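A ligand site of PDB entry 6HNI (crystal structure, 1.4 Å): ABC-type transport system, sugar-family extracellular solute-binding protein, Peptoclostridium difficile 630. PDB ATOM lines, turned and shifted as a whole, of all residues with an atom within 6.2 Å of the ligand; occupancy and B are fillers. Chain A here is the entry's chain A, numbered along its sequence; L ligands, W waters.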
ATOM      1  N   LEU A  31       9.044 -18.880  -0.796  1.00  0.00           N
ATOM      2  CA  LEU A  31       7.715 -18.393  -0.342  1.00  0.00           C
ATOM      3  C   LEU A  31       6.887 -17.700  -1.439  1.00  0.00           C
ATOM      4  O   LEU A  31       5.688 -17.972  -1.583  1.00  0.00           O
ATOM      5  CB  LEU A  31       7.950 -17.467   0.841  1.00  0.00           C
ATOM      6  CG  LEU A  31       6.707 -16.720   1.380  1.00  0.00           C
ATOM      7  CD1 LEU A  31       5.737 -17.748   1.883  1.00  0.00           C
ATOM      8  CD2 LEU A  31       7.198 -15.778   2.437  1.00  0.00           C
ATOM      9  N   HIS A  34       9.514 -12.113  -4.660  1.00  0.00           N
ATOM     10  CA  HIS A  34       9.887 -10.709  -4.406  1.00  0.00           C
ATOM     11  C   HIS A  34      11.408 -10.620  -4.672  1.00  0.00           C
ATOM     12  O   HIS A  34      12.070 -11.676  -4.664  1.00  0.00           O
ATOM     13  CB  HIS A  34       9.394 -10.099  -3.088  1.00  0.00           C
ATOM     14  CG  HIS A  34       9.981 -10.619  -1.794  1.00  0.00           C
ATOM     15  ND1 HIS A  34      11.214 -10.223  -1.319  1.00  0.00           N
ATOM     16  CD2 HIS A  34       9.423 -11.350  -0.797  1.00  0.00           C
ATOM     17  CE1 HIS A  34      11.397 -10.748  -0.117  1.00  0.00           C
ATOM     18  NE2 HIS A  34      10.314 -11.414   0.236  1.00  0.00           N
ATOM     19  N   ALA A  36      14.402  -9.992  -3.521  1.00  0.00           N
ATOM     20  CA  ALA A  36      15.449 -10.589  -2.710  1.00  0.00           C
ATOM     21  C   ALA A  36      15.362 -12.079  -2.804  1.00  0.00           C
ATOM     22  O   ALA A  36      16.393 -12.785  -2.888  1.00  0.00           O
ATOM     23  CB  ALA A  36      15.321 -10.141  -1.243  1.00  0.00           C
ATOM     24  N   LEU A  37      14.160 -12.634  -2.705  1.00  0.00           N
ATOM     25  CA  LEU A  37      14.055 -14.105  -2.730  1.00  0.00           C
ATOM     26  C   LEU A  37      14.447 -14.650  -4.077  1.00  0.00           C
ATOM     27  O   LEU A  37      15.166 -15.681  -4.137  1.00  0.00           O
ATOM     28  CB  LEU A  37      12.655 -14.577  -2.338  1.00  0.00           C
ATOM     29  CG  LEU A  37      12.092 -14.015  -1.010  1.00  0.00           C
ATOM     30  CD1 LEU A  37      10.870 -14.785  -0.606  1.00  0.00           C
ATOM     31  CD2 LEU A  37      13.098 -14.004   0.130  1.00  0.00           C
ATOM     32  N   ILE A  91      13.960 -20.820   0.979  1.00  0.00           N
ATOM     33  CA  ILE A  91      14.185 -19.426   0.785  1.00  0.00           C
ATOM     34  C   ILE A  91      13.071 -18.700   1.559  1.00  0.00           C
ATOM     35  O   ILE A  91      11.923 -18.740   1.118  1.00  0.00           O
ATOM     36  CB  ILE A  91      14.150 -19.034  -0.702  1.00  0.00           C
ATOM     37  CG1 ILE A  91      15.212 -19.829  -1.513  1.00  0.00           C
ATOM     38  CG2 ILE A  91      14.316 -17.545  -0.898  1.00  0.00           C
ATOM     39  CD1 ILE A  91      14.995 -19.638  -2.979  1.00  0.00           C
ATOM     40  N   SER A  92      13.520 -18.021   2.620  1.00  0.00           N
ATOM     41  CA  SER A  92      12.686 -17.273   3.626  1.00  0.00           C
ATOM     42  C   SER A  92      12.437 -18.090   4.863  1.00  0.00           C
ATOM     43  O   SER A  92      12.395 -19.325   4.864  1.00  0.00           O
ATOM     44  CB  SER A  92      11.357 -16.764   3.073  1.00  0.00           C
ATOM     45  OG  SER A  92      10.369 -17.776   3.117  1.00  0.00           O
ATOM     46  N   THR A  93      12.096 -17.350   5.962  1.00  0.00           N
ATOM     47  CA  THR A  93      11.770 -17.962   7.224  1.00  0.00           C
ATOM     48  C   THR A  93      10.577 -18.902   7.131  1.00  0.00           C
ATOM     49  O   THR A  93      10.626 -20.016   7.609  1.00  0.00           O
ATOM     50  CB  THR A  93      11.685 -16.931   8.362  1.00  0.00           C
ATOM     51  OG1 THR A  93      12.949 -16.322   8.554  1.00  0.00           O
ATOM     52  CG2 THR A  93      11.229 -17.556   9.656  1.00  0.00           C
ATOM     53  N   PRO A  94       9.420 -18.411   6.620  1.00  0.00           N
ATOM     54  CA  PRO A  94       8.287 -19.343   6.507  1.00  0.00           C
ATOM     55  C   PRO A  94       8.563 -20.636   5.709  1.00  0.00           C
ATOM     56  O   PRO A  94       8.130 -21.734   6.143  1.00  0.00           O
ATOM     57  CB  PRO A  94       7.169 -18.471   5.885  1.00  0.00           C
ATOM     58  CG  PRO A  94       7.575 -17.070   6.205  1.00  0.00           C
ATOM     59  CD  PRO A  94       9.082 -17.082   6.100  1.00  0.00           C
ATOM     60  N   THR A 111      18.280 -19.741   3.182  1.00  0.00           N
ATOM     61  CA  THR A 111      18.801 -18.431   2.897  1.00  0.00           C
ATOM     62  C   THR A 111      17.640 -17.423   3.166  1.00  0.00           C
ATOM     63  O   THR A 111      16.460 -17.846   3.292  1.00  0.00           O
ATOM     64  CB  THR A 111      19.267 -18.222   1.464  1.00  0.00           C
ATOM     65  OG1 THR A 111      20.015 -16.980   1.350  1.00  0.00           O
ATOM     66  CG2 THR A 111      18.165 -18.290   0.433  1.00  0.00           C
ATOM     67  N   ALA A 112      18.026 -16.160   3.261  1.00  0.00           N
ATOM     68  CA  ALA A 112      17.014 -15.045   3.493  1.00  0.00           C
ATOM     69  C   ALA A 112      16.240 -15.328   4.747  1.00  0.00           C
ATOM     70  O   ALA A 112      15.033 -15.007   4.772  1.00  0.00           O
ATOM     71  CB  ALA A 112      16.128 -14.907   2.306  1.00  0.00           C
ATOM     72  N   VAL A 113      16.887 -15.836   5.770  1.00  0.00           N
ATOM     73  CA  VAL A 113      16.317 -16.054   7.100  1.00  0.00           C
ATOM     74  C   VAL A 113      16.993 -15.108   8.038  1.00  0.00           C
ATOM     75  O   VAL A 113      18.183 -15.136   8.268  1.00  0.00           O
ATOM     76  CB  VAL A 113      16.482 -17.500   7.571  1.00  0.00           C
ATOM     77  CG1 VAL A 113      16.098 -17.694   9.034  1.00  0.00           C
ATOM     78  CG2 VAL A 113      15.708 -18.419   6.674  1.00  0.00           C
ATOM     79  N   SER A 114      16.205 -14.182   8.660  1.00  0.00           N
ATOM     80  CA  SER A 114      16.796 -13.140   9.449  1.00  0.00           C
ATOM     81  C   SER A 114      17.462 -13.618  10.706  1.00  0.00           C
ATOM     82  O   SER A 114      18.522 -13.127  11.080  1.00  0.00           O
ATOM     83  CB  SER A 114      15.731 -12.071   9.851  1.00  0.00           C
ATOM     84  OG  SER A 114      15.142 -11.484   8.745  1.00  0.00           O
ATOM     85  N   ASP A 115      16.800 -14.541  11.394  1.00  0.00           N
ATOM     86  CA  ASP A 115      17.180 -15.007  12.748  1.00  0.00           C
ATOM     87  C   ASP A 115      16.850 -16.480  12.844  1.00  0.00           C
ATOM     88  O   ASP A 115      15.790 -16.921  13.242  1.00  0.00           O
ATOM     89  CB  ASP A 115      16.490 -14.197  13.841  1.00  0.00           C
ATOM     90  CG  ASP A 115      17.164 -14.363  15.236  1.00  0.00           C
ATOM     91  OD1 ASP A 115      17.578 -15.508  15.604  1.00  0.00           O
ATOM     92  OD2 ASP A 115      17.192 -13.353  15.970  1.00  0.00           O
ATOM     93  N   ASP A 137      20.125 -13.517   6.377  1.00  0.00           N
ATOM     94  CA  ASP A 137      20.097 -12.155   5.865  1.00  0.00           C
ATOM     95  C   ASP A 137      20.000 -11.138   6.984  1.00  0.00           C
ATOM     96  O   ASP A 137      19.501 -10.003   6.740  1.00  0.00           O
ATOM     97  CB  ASP A 137      19.016 -11.909   4.802  1.00  0.00           C
ATOM     98  CG  ASP A 137      17.575 -12.043   5.350  1.00  0.00           C
ATOM     99  OD1 ASP A 137      17.413 -12.608   6.438  1.00  0.00           O
ATOM    100  OD2 ASP A 137      16.668 -11.614   4.567  1.00  0.00           O
ATOM    101  N   GLU A 166       5.302 -13.147  11.363  1.00  0.00           N
ATOM    102  CA  GLU A 166       6.664 -13.440  10.947  1.00  0.00           C
ATOM    103  C   GLU A 166       7.642 -13.186  12.085  1.00  0.00           C
ATOM    104  O   GLU A 166       7.889 -12.025  12.494  1.00  0.00           O
ATOM    105  CB  GLU A 166       7.033 -12.619   9.697  1.00  0.00           C
ATOM    106  CG  GLU A 166       6.327 -13.070   8.405  1.00  0.00           C
ATOM    107  CD  GLU A 166       6.716 -12.249   7.154  1.00  0.00           C
ATOM    108  OE1 GLU A 166       7.940 -12.025   6.928  1.00  0.00           O
ATOM    109  OE2 GLU A 166       5.778 -11.825   6.380  1.00  0.00           O
ATOM    110  N   ASN A 168      10.820 -13.333  11.986  1.00  0.00           N
ATOM    111  CA  ASN A 168      11.836 -12.469  11.424  1.00  0.00           C
ATOM    112  C   ASN A 168      11.556 -10.982  11.586  1.00  0.00           C
ATOM    113  O   ASN A 168      12.447 -10.205  11.908  1.00  0.00           O
ATOM    114  CB  ASN A 168      12.135 -12.788   9.942  1.00  0.00           C
ATOM    115  CG  ASN A 168      10.860 -12.921   9.099  1.00  0.00           C
ATOM    116  OD1 ASN A 168      10.147 -13.920   9.289  1.00  0.00           O
ATOM    117  ND2 ASN A 168      10.602 -12.014   8.182  1.00  0.00           N
ATOM    118  N   GLN A 172      13.201  -7.834  14.232  1.00  0.00           N
ATOM    119  CA  GLN A 172      13.651  -6.576  13.692  1.00  0.00           C
ATOM    120  C   GLN A 172      12.907  -5.360  14.325  1.00  0.00           C
ATOM    121  O   GLN A 172      13.546  -4.339  14.574  1.00  0.00           O
ATOM    122  CB  GLN A 172      13.452  -6.566  12.181  1.00  0.00           C
ATOM    123  CG  GLN A 172      14.435  -7.548  11.463  1.00  0.00           C
ATOM    124  CD  GLN A 172      14.175  -7.650   9.973  1.00  0.00           C
ATOM    125  OE1 GLN A 172      14.464  -6.743   9.209  1.00  0.00           O
ATOM    126  NE2 GLN A 172      13.599  -8.786   9.578  1.00  0.00           N
ATOM    127  N   VAL A 214      11.096  -0.161   6.530  1.00  0.00           N
ATOM    128  CA  VAL A 214      10.595  -1.442   6.063  1.00  0.00           C
ATOM    129  C   VAL A 214      11.600  -2.534   6.428  1.00  0.00           C
ATOM    130  O   VAL A 214      12.664  -2.647   5.768  1.00  0.00           O
ATOM    131  CB  VAL A 214      10.257  -1.401   4.586  1.00  0.00           C
ATOM    132  CG1 VAL A 214       9.764  -2.752   4.080  1.00  0.00           C
ATOM    133  CG2 VAL A 214       9.215  -0.302   4.295  1.00  0.00           C
ATOM    134  N   PRO A 215      11.292  -3.340   7.422  1.00  0.00           N
ATOM    135  CA  PRO A 215      12.164  -4.495   7.722  1.00  0.00           C
ATOM    136  C   PRO A 215      12.060  -5.528   6.601  1.00  0.00           C
ATOM    137  O   PRO A 215      11.343  -5.384   5.641  1.00  0.00           O
ATOM    138  CB  PRO A 215      11.590  -5.056   9.032  1.00  0.00           C
ATOM    139  CG  PRO A 215      10.314  -4.371   9.251  1.00  0.00           C
ATOM    140  CD  PRO A 215      10.020  -3.408   8.172  1.00  0.00           C
ATOM    141  N   THR A 216      12.897  -6.573   6.746  1.00  0.00           N
ATOM    142  CA  THR A 216      12.790  -7.723   5.835  1.00  0.00           C
ATOM    143  C   THR A 216      11.615  -8.644   6.199  1.00  0.00           C
ATOM    144  O   THR A 216      11.749  -9.696   6.788  1.00  0.00           O
ATOM    145  CB  THR A 216      14.139  -8.497   5.690  1.00  0.00           C
ATOM    146  OG1 THR A 216      14.501  -9.091   6.904  1.00  0.00           O
ATOM    147  CG2 THR A 216      15.197  -7.559   5.157  1.00  0.00           C
ATOM    148  N   ASP A 217      10.410  -8.061   5.958  1.00  0.00           N
ATOM    149  CA  ASP A 217       9.131  -8.650   6.143  1.00  0.00           C
ATOM    150  C   ASP A 217       8.543  -9.041   4.778  1.00  0.00           C
ATOM    151  O   ASP A 217       8.465  -8.226   3.872  1.00  0.00           O
ATOM    152  CB  ASP A 217       8.215  -7.548   6.765  1.00  0.00           C
ATOM    153  CG  ASP A 217       6.831  -8.066   7.074  1.00  0.00           C
ATOM    154  OD1 ASP A 217       5.945  -8.112   6.197  1.00  0.00           O
ATOM    155  OD2 ASP A 217       6.634  -8.437   8.248  1.00  0.00           O
ATOM    156  N   ASN A 218       8.245 -10.351   4.620  1.00  0.00           N
ATOM    157  CA  ASN A 218       7.800 -10.856   3.370  1.00  0.00           C
ATOM    158  C   ASN A 218       6.475 -10.287   2.873  1.00  0.00           C
ATOM    159  O   ASN A 218       6.302 -10.043   1.721  1.00  0.00           O
ATOM    160  CB  ASN A 218       7.737 -12.396   3.385  1.00  0.00           C
ATOM    161  CG  ASN A 218       9.117 -13.044   3.526  1.00  0.00           C
ATOM    162  OD1 ASN A 218       9.910 -13.033   2.555  1.00  0.00           O
ATOM    163  ND2 ASN A 218       9.399 -13.563   4.693  1.00  0.00           N
ATOM    164  N   ALA A 221       7.192  -6.519   1.900  1.00  0.00           N
ATOM    165  CA  ALA A 221       8.014  -6.511   0.686  1.00  0.00           C
ATOM    166  C   ALA A 221       7.212  -6.887  -0.550  1.00  0.00           C
ATOM    167  O   ALA A 221       7.514  -6.409  -1.633  1.00  0.00           O
ATOM    168  CB  ALA A 221       9.225  -7.446   0.879  1.00  0.00           C
ATOM    169  N   ALA A 241      15.191  -2.108   4.492  1.00  0.00           N
ATOM    170  CA  ALA A 241      16.362  -2.884   4.937  1.00  0.00           C
ATOM    171  C   ALA A 241      17.233  -3.402   3.782  1.00  0.00           C
ATOM    172  O   ALA A 241      18.421  -3.632   4.026  1.00  0.00           O
ATOM    173  CB  ALA A 241      15.925  -4.031   5.790  1.00  0.00           C
ATOM    174  N   GLU A 242      16.684  -3.542   2.601  1.00  0.00           N
ATOM    175  CA  GLU A 242      17.414  -4.058   1.430  1.00  0.00           C
ATOM    176  C   GLU A 242      16.859  -3.509   0.163  1.00  0.00           C
ATOM    177  O   GLU A 242      15.877  -2.748   0.208  1.00  0.00           O
ATOM    178  CB  GLU A 242      17.481  -5.587   1.459  1.00  0.00           C
ATOM    179  CG  GLU A 242      16.162  -6.322   1.415  1.00  0.00           C
ATOM    180  CD  GLU A 242      15.653  -6.695   0.034  1.00  0.00           C
ATOM    181  OE1 GLU A 242      16.445  -6.634  -0.966  1.00  0.00           O
ATOM    182  OE2 GLU A 242      14.454  -7.071  -0.088  1.00  0.00           O
ATOM    183  N   GLY A 244      15.444  -4.667  -2.700  1.00  0.00           N
ATOM    184  CA  GLY A 244      14.251  -5.084  -3.406  1.00  0.00           C
ATOM    185  C   GLY A 244      13.126  -4.053  -3.263  1.00  0.00           C
ATOM    186  O   GLY A 244      12.530  -3.609  -4.255  1.00  0.00           O
ATOM    187  N   PRO A 245      12.808  -3.665  -2.028  1.00  0.00           N
ATOM    188  CA  PRO A 245      11.731  -2.646  -1.906  1.00  0.00           C
ATOM    189  C   PRO A 245      12.088  -1.320  -2.542  1.00  0.00           C
ATOM    190  O   PRO A 245      11.198  -0.594  -2.955  1.00  0.00           O
ATOM    191  CB  PRO A 245      11.602  -2.523  -0.390  1.00  0.00           C
ATOM    192  CG  PRO A 245      11.930  -3.897   0.128  1.00  0.00           C
ATOM    193  CD  PRO A 245      13.051  -4.362  -0.765  1.00  0.00           C
ATOM    194  N   TYR A 258      21.652 -10.046  -2.140  1.00  0.00           N
ATOM    195  CA  TYR A 258      20.997 -11.340  -1.956  1.00  0.00           C
ATOM    196  C   TYR A 258      21.437 -12.406  -2.988  1.00  0.00           C
ATOM    197  O   TYR A 258      21.459 -13.589  -2.651  1.00  0.00           O
ATOM    198  CB  TYR A 258      19.476 -11.157  -1.974  1.00  0.00           C
ATOM    199  CG  TYR A 258      18.913 -10.777  -0.609  1.00  0.00           C
ATOM    200  CD1 TYR A 258      18.974  -9.441  -0.154  1.00  0.00           C
ATOM    201  CD2 TYR A 258      18.357 -11.697   0.214  1.00  0.00           C
ATOM    202  CE1 TYR A 258      18.475  -9.113   1.076  1.00  0.00           C
ATOM    203  CE2 TYR A 258      17.789 -11.343   1.462  1.00  0.00           C
ATOM    204  CZ  TYR A 258      17.897 -10.036   1.865  1.00  0.00           C
ATOM    205  OH  TYR A 258      17.338  -9.636   3.091  1.00  0.00           O
HETATM  206  N1  LIG L   1      14.281 -11.898   6.036  1.00  0.00           N
HETATM  207  C1  LIG L   1      13.044 -12.520   5.515  1.00  0.00           C
HETATM  208  C2  LIG L   1      12.800 -13.843   6.241  1.00  0.00           C
HETATM  209  O1  LIG L   1      11.917 -14.572   5.831  1.00  0.00           O
HETATM  210  C3  LIG L   1      13.022 -12.600   3.971  1.00  0.00           C
HETATM  211  C4  LIG L   1      12.970 -11.251   3.338  1.00  0.00           C
HETATM  212  C5  LIG L   1      11.812 -10.439   3.487  1.00  0.00           C
HETATM  213  C6  LIG L   1      14.018 -10.704   2.645  1.00  0.00           C
HETATM  214  C7  LIG L   1      11.793  -9.168   2.970  1.00  0.00           C
HETATM  215  C8  LIG L   1      14.009  -9.428   2.119  1.00  0.00           C
HETATM  216  C9  LIG L   1      12.853  -8.635   2.302  1.00  0.00           C
HETATM  217  O2  LIG L   1      12.824  -7.341   1.787  1.00  0.00           O
HETATM  218  O3  LIG L   1      13.418 -14.095   7.259  1.00  0.00           O
HETATM  219  O   HOH W   1      13.300  -4.728   3.340  1.00  0.00           O
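The side-chain carboxylate (OE2) of Glu 242 is in hydrogen-bond range of an oxygen (O2) of the ligand, at 2.5 Å.
N of Thr 93 lies within hydrogen-bond range of O1 of the ligand, 2.8 Å away.
OG1 of Thr 93 lies within hydrogen-bond range of O3 of the ligand (2.6 Å).
A nitrogen (N1) of the ligand lies within salt-bridge range of the side-chain carboxylate of Asp 137, 2.8 Å away.
The backbone NH (N) of Ser 114 sits at hydrogen-bond distance from an oxygen (O3) of the ligand.
OG of Ser 114 sits at hydrogen-bond distance from N1 of the ligand.
The backbone carbonyl oxygen (O) of Ala 112 sits close to a nitrogen (N1) of the ligand (3.4 Å).
ND2 of Asn 218 is in hydrogen-bond range of O1 of the ligand (2.9 Å).
A nitrogen (N1) of the ligand sits close to the backbone carbonyl oxygen of Thr 216 (3.4 Å).
A nitrogen (N1) of the ligand is in hydrogen-bond range of the side-chain hydroxyl (OG1) of Thr 216, 2.9 Å away.
Water W1 lies within hydrogen-bond range of an oxygen (O2) of the ligand (3.1 Å), the backbone carbonyl oxygen (O) of Pro 215 (3.1 Å), the backbone carbonyl oxygen (O) of Val 214 (3.3 Å) and the backbone NH (N) of Ala 241 (3.4 Å).
CE1 of His 34 touches C7 of the ligand, at 3.5 Å.
Ala 36 touches the ligand.
Ser 92 touches the ligand (CB to O1, 3.6 Å).
Pro 94 touches the ligand (CD to O1, 3.8 Å).
CA of Val 113 touches O3 of the ligand, 3.5 Å away.
Asn 168 touches the ligand (CB to O3, 3.2 Å).
Asp 217 touches the ligand.
Ala 221 touches the ligand (CB to O2, 3.7 Å).
CG of Pro 245 touches O2 of the ligand, at 3.9 Å.
Tyr 258 touches the ligand (OH to C8, 3.5 Å).
Hydrophobic or aromatic side chains within 4 Å of the ligand: His 34, Ala 36, Pro 94, Ala 221, Pro 245 and Tyr 258.
Of the 28 residues printed, 17 come within 4 Å of the ligand.
The side-chain carboxylate (OD1) of Asp 137 is in hydrogen-bond range of the backbone NH (N) of Ser 114, 3.0 Å away.
The side-chain hydroxyl of Tyr 258 lies within hydrogen-bond range of the side-chain carboxylate of Asp 137 (2.6 Å).
N of Asp 137 is in hydrogen-bond range of O of Val 113 (3.2 Å).
The backbone NH (N) of Asn 218 sits at hydrogen-bond distance from the side-chain carboxylate (OE1) of Glu 166, 2.9 Å away.
The backbone carbonyl oxygen (O) of Thr 216 sits at hydrogen-bond distance from the side-chain amide nitrogen (ND2) of Asn 168, 2.9 Å away.
The side-chain hydroxyl (OG1) of Thr 216 is in hydrogen-bond range of the side-chain amide nitrogen (NE2) of Gln 172, 2.8 Å away.
O of Asn 168 sits at hydrogen-bond distance from NE2 of Gln 172 (3.0 Å).
The side-chain amide nitrogen (ND2) of Asn 168 lies within hydrogen-bond range of the side-chain carboxylate (OE1) of Glu 166, at 2.9 Å.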
